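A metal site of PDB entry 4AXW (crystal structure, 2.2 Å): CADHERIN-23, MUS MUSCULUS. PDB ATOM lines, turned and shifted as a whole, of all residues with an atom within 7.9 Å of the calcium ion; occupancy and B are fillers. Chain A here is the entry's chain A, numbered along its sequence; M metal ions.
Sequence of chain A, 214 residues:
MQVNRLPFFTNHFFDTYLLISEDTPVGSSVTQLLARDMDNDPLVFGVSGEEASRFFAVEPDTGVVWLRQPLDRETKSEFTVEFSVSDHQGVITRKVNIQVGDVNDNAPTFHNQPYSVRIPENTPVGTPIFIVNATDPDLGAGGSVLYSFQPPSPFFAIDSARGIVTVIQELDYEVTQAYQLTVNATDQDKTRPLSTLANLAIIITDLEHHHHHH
The side-chain carboxylate (OD1) of Asp 87 lies within hydrogen-bond range of the backbone NH (N) of Gln 89, at 2.9 Å. The side-chain amide oxygen (OD1) of Asn 4 sits close to the side-chain amide nitrogen (NE2) of Gln 89 (3.5 Å). The side-chain carboxylate of Asp 87 is in hydrogen-bond range of the backbone NH of Gly 90.
Of the 18 residues printed, 6 come within 4 Å of the calcium ion. The nearest printed residue that does not touch the calcium ion is Leu 6 (4.5 Å).
The calcium ion is bound by the side-chain carboxylate (OD2) of Asp 41. O of Arg 5 binds the calcium ion, 2.3 Å away. The side-chain carboxylate (OD2) of Asp 39 binds the calcium ion, at 2.3 Å. OD2 of Asp 87 binds the calcium ion (2.3 Å). The calcium ion is bound by the side-chain amide oxygen (OD1) of Asn 4. The side-chain carboxylate (OD1) of Asp 37 is bound to the calcium ion. The side-chain carboxylate (OD2) of Asp 37 binds the calcium ion, 2.6 Å away. The calcium ion has seven donor atoms within binding distance.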
ATOM      1  N   VAL A   3      -7.135  -4.011   6.640  1.00  0.00           N
ATOM      2  CA  VAL A   3      -7.452  -2.668   7.139  1.00  0.00           C
ATOM      3  C   VAL A   3      -6.387  -1.721   6.572  1.00  0.00           C
ATOM      4  O   VAL A   3      -5.259  -2.128   6.284  1.00  0.00           O
ATOM      5  CB  VAL A   3      -7.538  -2.587   8.738  1.00  0.00           C
ATOM      6  CG1 VAL A   3      -8.712  -3.478   9.249  1.00  0.00           C
ATOM      7  CG2 VAL A   3      -6.221  -2.981   9.425  1.00  0.00           C
ATOM      8  N   ASN A   4      -6.755  -0.453   6.351  1.00  0.00           N
ATOM      9  CA  ASN A   4      -5.753   0.537   5.953  1.00  0.00           C
ATOM     10  C   ASN A   4      -4.648   0.644   6.992  1.00  0.00           C
ATOM     11  O   ASN A   4      -4.921   0.579   8.179  1.00  0.00           O
ATOM     12  CB  ASN A   4      -6.354   1.901   5.788  1.00  0.00           C
ATOM     13  CG  ASN A   4      -5.320   2.914   5.275  1.00  0.00           C
ATOM     14  OD1 ASN A   4      -4.592   2.646   4.325  1.00  0.00           O
ATOM     15  ND2 ASN A   4      -5.249   4.058   5.943  1.00  0.00           N
ATOM     16  N   ARG A   5      -3.412   0.774   6.518  1.00  0.00           N
ATOM     17  CA  ARG A   5      -2.311   1.216   7.381  1.00  0.00           C
ATOM     18  C   ARG A   5      -1.976   2.675   7.116  1.00  0.00           C
ATOM     19  O   ARG A   5      -1.944   3.135   5.971  1.00  0.00           O
ATOM     20  CB  ARG A   5      -1.106   0.278   7.195  1.00  0.00           C
ATOM     21  CG  ARG A   5      -1.368  -1.049   7.903  1.00  0.00           C
ATOM     22  CD  ARG A   5      -0.783  -2.250   7.208  1.00  0.00           C
ATOM     23  NE  ARG A   5      -1.249  -2.442   5.849  1.00  0.00           N
ATOM     24  CZ  ARG A   5      -0.619  -3.221   4.966  1.00  0.00           C
ATOM     25  NH1 ARG A   5       0.487  -3.892   5.328  1.00  0.00           N
ATOM     26  NH2 ARG A   5      -1.073  -3.331   3.724  1.00  0.00           N
ATOM     27  N   LEU A   6      -1.828   3.441   8.182  1.00  0.00           N
ATOM     28  CA  LEU A   6      -1.552   4.851   8.065  1.00  0.00           C
ATOM     29  C   LEU A   6      -0.073   5.014   7.642  1.00  0.00           C
ATOM     30  O   LEU A   6       0.798   4.158   7.966  1.00  0.00           O
ATOM     31  CB  LEU A   6      -1.861   5.566   9.399  1.00  0.00           C
ATOM     32  CG  LEU A   6      -3.362   5.689   9.738  1.00  0.00           C
ATOM     33  CD1 LEU A   6      -3.674   6.043  11.201  1.00  0.00           C
ATOM     34  CD2 LEU A   6      -4.064   6.665   8.821  1.00  0.00           C
ATOM     35  N   PRO A   7       0.223   6.105   6.906  1.00  0.00           N
ATOM     36  CA  PRO A   7       1.592   6.411   6.512  1.00  0.00           C
ATOM     37  C   PRO A   7       2.431   6.822   7.702  1.00  0.00           C
ATOM     38  O   PRO A   7       1.880   7.161   8.719  1.00  0.00           O
ATOM     39  CB  PRO A   7       1.430   7.595   5.559  1.00  0.00           C
ATOM     40  CG  PRO A   7       0.195   8.269   5.995  1.00  0.00           C
ATOM     41  CD  PRO A   7      -0.703   7.161   6.502  1.00  0.00           C
ATOM     42  N   ARG A  36       6.424   6.729   4.017  1.00  0.00           N
ATOM     43  CA  ARG A  36       6.129   5.418   3.411  1.00  0.00           C
ATOM     44  C   ARG A  36       4.719   5.013   3.853  1.00  0.00           C
ATOM     45  O   ARG A  36       4.197   5.490   4.875  1.00  0.00           O
ATOM     46  CB  ARG A  36       7.083   4.332   3.917  1.00  0.00           C
ATOM     47  CG  ARG A  36       8.597   4.500   3.611  1.00  0.00           C
ATOM     48  CD  ARG A  36       8.925   4.582   2.107  1.00  0.00           C
ATOM     49  NE  ARG A  36       8.720   3.327   1.386  1.00  0.00           N
ATOM     50  CZ  ARG A  36       8.693   3.213   0.049  1.00  0.00           C
ATOM     51  NH1 ARG A  36       8.897   4.276  -0.733  1.00  0.00           N
ATOM     52  NH2 ARG A  36       8.478   2.023  -0.512  1.00  0.00           N
ATOM     53  N   ASP A  37       4.099   4.106   3.113  1.00  0.00           N
ATOM     54  CA  ASP A  37       2.780   3.609   3.441  1.00  0.00           C
ATOM     55  C   ASP A  37       2.804   2.160   3.004  1.00  0.00           C
ATOM     56  O   ASP A  37       3.205   1.879   1.906  1.00  0.00           O
ATOM     57  CB  ASP A  37       1.716   4.365   2.653  1.00  0.00           C
ATOM     58  CG  ASP A  37       0.303   4.021   3.071  1.00  0.00           C
ATOM     59  OD1 ASP A  37      -0.207   2.957   2.646  1.00  0.00           O
ATOM     60  OD2 ASP A  37      -0.353   4.898   3.735  1.00  0.00           O
ATOM     61  N   MET A  38       2.391   1.242   3.875  1.00  0.00           N
ATOM     62  CA  MET A  38       2.567  -0.184   3.573  1.00  0.00           C
ATOM     63  C   MET A  38       1.614  -0.647   2.505  1.00  0.00           C
ATOM     64  O   MET A  38       1.814  -1.698   1.930  1.00  0.00           O
ATOM     65  CB  MET A  38       2.386  -1.027   4.835  1.00  0.00           C
ATOM     66  CG  MET A  38       3.533  -0.876   5.869  1.00  0.00           C
ATOM     67  SD  MET A  38       5.147  -1.623   5.389  1.00  0.00           S
ATOM     68  CE  MET A  38       6.082  -0.148   4.973  1.00  0.00           C
ATOM     69  N   ASP A  39       0.553   0.120   2.261  1.00  0.00           N
ATOM     70  CA  ASP A  39      -0.401  -0.185   1.179  1.00  0.00           C
ATOM     71  C   ASP A  39       0.085   0.387  -0.155  1.00  0.00           C
ATOM     72  O   ASP A  39      -0.533   0.150  -1.183  1.00  0.00           O
ATOM     73  CB  ASP A  39      -1.796   0.380   1.527  1.00  0.00           C
ATOM     74  CG  ASP A  39      -2.227   0.105   2.978  1.00  0.00           C
ATOM     75  OD1 ASP A  39      -2.471  -1.075   3.327  1.00  0.00           O
ATOM     76  OD2 ASP A  39      -2.363   1.090   3.759  1.00  0.00           O
ATOM     77  N   ASN A  40       1.191   1.139  -0.140  1.00  0.00           N
ATOM     78  CA  ASN A  40       1.702   1.888  -1.303  1.00  0.00           C
ATOM     79  C   ASN A  40       0.754   2.999  -1.772  1.00  0.00           C
ATOM     80  O   ASN A  40       0.708   3.351  -2.934  1.00  0.00           O
ATOM     81  CB  ASN A  40       2.145   0.981  -2.457  1.00  0.00           C
ATOM     82  CG  ASN A  40       3.447   0.251  -2.153  1.00  0.00           C
ATOM     83  OD1 ASN A  40       4.551   0.834  -2.132  1.00  0.00           O
ATOM     84  ND2 ASN A  40       3.343  -1.008  -1.935  1.00  0.00           N
ATOM     85  N   ASP A  41       0.028   3.548  -0.820  1.00  0.00           N
ATOM     86  CA  ASP A  41      -0.866   4.648  -1.096  1.00  0.00           C
ATOM     87  C   ASP A  41      -0.086   5.886  -1.521  1.00  0.00           C
ATOM     88  O   ASP A  41       0.981   6.184  -0.990  1.00  0.00           O
ATOM     89  CB  ASP A  41      -1.704   4.960   0.162  1.00  0.00           C
ATOM     90  CG  ASP A  41      -2.694   3.868   0.490  1.00  0.00           C
ATOM     91  OD1 ASP A  41      -3.106   3.182  -0.438  1.00  0.00           O
ATOM     92  OD2 ASP A  41      -3.034   3.674   1.656  1.00  0.00           O
ATOM     93  N   PRO A  42      -0.640   6.618  -2.492  1.00  0.00           N
ATOM     94  CA  PRO A  42      -0.044   7.910  -2.826  1.00  0.00           C
ATOM     95  C   PRO A  42      -0.341   8.895  -1.702  1.00  0.00           C
ATOM     96  O   PRO A  42      -1.417   8.812  -1.066  1.00  0.00           O
ATOM     97  CB  PRO A  42      -0.695   8.280  -4.163  1.00  0.00           C
ATOM     98  CG  PRO A  42      -1.948   7.495  -4.270  1.00  0.00           C
ATOM     99  CD  PRO A  42      -1.815   6.280  -3.325  1.00  0.00           C
ATOM    100  N   LEU A  43       0.628   9.759  -1.387  1.00  0.00           N
ATOM    101  CA  LEU A  43       0.602  10.536  -0.137  1.00  0.00           C
ATOM    102  C   LEU A  43       0.489  12.007  -0.445  1.00  0.00           C
ATOM    103  O   LEU A  43       1.107  12.466  -1.390  1.00  0.00           O
ATOM    104  CB  LEU A  43       1.867  10.281   0.679  1.00  0.00           C
ATOM    105  CG  LEU A  43       2.090   8.816   1.050  1.00  0.00           C
ATOM    106  CD1 LEU A  43       3.302   8.639   1.894  1.00  0.00           C
ATOM    107  CD2 LEU A  43       0.813   8.287   1.801  1.00  0.00           C
ATOM    108  N   SER A  86      -0.905  12.389   4.604  1.00  0.00           N
ATOM    109  CA  SER A  86      -2.181  11.720   4.511  1.00  0.00           C
ATOM    110  C   SER A  86      -2.164  10.733   3.377  1.00  0.00           C
ATOM    111  O   SER A  86      -1.704  11.088   2.303  1.00  0.00           O
ATOM    112  CB  SER A  86      -3.280  12.765   4.223  1.00  0.00           C
ATOM    113  OG  SER A  86      -4.489  12.108   3.847  1.00  0.00           O
ATOM    114  N   ASP A  87      -2.737   9.541   3.588  1.00  0.00           N
ATOM    115  CA  ASP A  87      -3.054   8.583   2.492  1.00  0.00           C
ATOM    116  C   ASP A  87      -4.510   8.633   1.987  1.00  0.00           C
ATOM    117  O   ASP A  87      -4.953   7.704   1.365  1.00  0.00           O
ATOM    118  CB  ASP A  87      -2.721   7.142   2.881  1.00  0.00           C
ATOM    119  CG  ASP A  87      -3.636   6.583   4.009  1.00  0.00           C
ATOM    120  OD1 ASP A  87      -4.619   7.282   4.385  1.00  0.00           O
ATOM    121  OD2 ASP A  87      -3.366   5.419   4.495  1.00  0.00           O
ATOM    122  N   HIS A  88      -5.222   9.709   2.283  1.00  0.00           N
ATOM    123  CA  HIS A  88      -6.647   9.879   1.920  1.00  0.00           C
ATOM    124  C   HIS A  88      -7.677   9.139   2.837  1.00  0.00           C
ATOM    125  O   HIS A  88      -8.894   9.381   2.708  1.00  0.00           O
ATOM    126  CB  HIS A  88      -6.940   9.514   0.442  1.00  0.00           C
ATOM    127  CG  HIS A  88      -5.993  10.118  -0.548  1.00  0.00           C
ATOM    128  ND1 HIS A  88      -6.044  11.450  -0.933  1.00  0.00           N
ATOM    129  CD2 HIS A  88      -4.985   9.562  -1.281  1.00  0.00           C
ATOM    130  CE1 HIS A  88      -5.117  11.687  -1.835  1.00  0.00           C
ATOM    131  NE2 HIS A  88      -4.457  10.559  -2.064  1.00  0.00           N
ATOM    132  N   GLN A  89      -7.228   8.302   3.757  1.00  0.00           N
ATOM    133  CA  GLN A  89      -8.137   7.731   4.734  1.00  0.00           C
ATOM    134  C   GLN A  89      -7.840   8.261   6.094  1.00  0.00           C
ATOM    135  O   GLN A  89      -8.740   8.514   6.864  1.00  0.00           O
ATOM    136  CB  GLN A  89      -8.106   6.210   4.704  1.00  0.00           C
ATOM    137  CG  GLN A  89      -8.548   5.683   3.347  1.00  0.00           C
ATOM    138  CD  GLN A  89      -8.557   4.159   3.272  1.00  0.00           C
ATOM    139  OE1 GLN A  89      -9.506   3.498   3.739  1.00  0.00           O
ATOM    140  NE2 GLN A  89      -7.502   3.585   2.650  1.00  0.00           N
ATOM    141  N   GLY A  90      -6.580   8.505   6.401  1.00  0.00           N
ATOM    142  CA  GLY A  90      -6.238   9.173   7.654  1.00  0.00           C
ATOM    143  C   GLY A  90      -5.095  10.141   7.463  1.00  0.00           C
ATOM    144  O   GLY A  90      -4.399  10.084   6.463  1.00  0.00           O
HETATM  145 CA    CA M   1      -2.429   3.417   3.756  1.00  0.00          CA
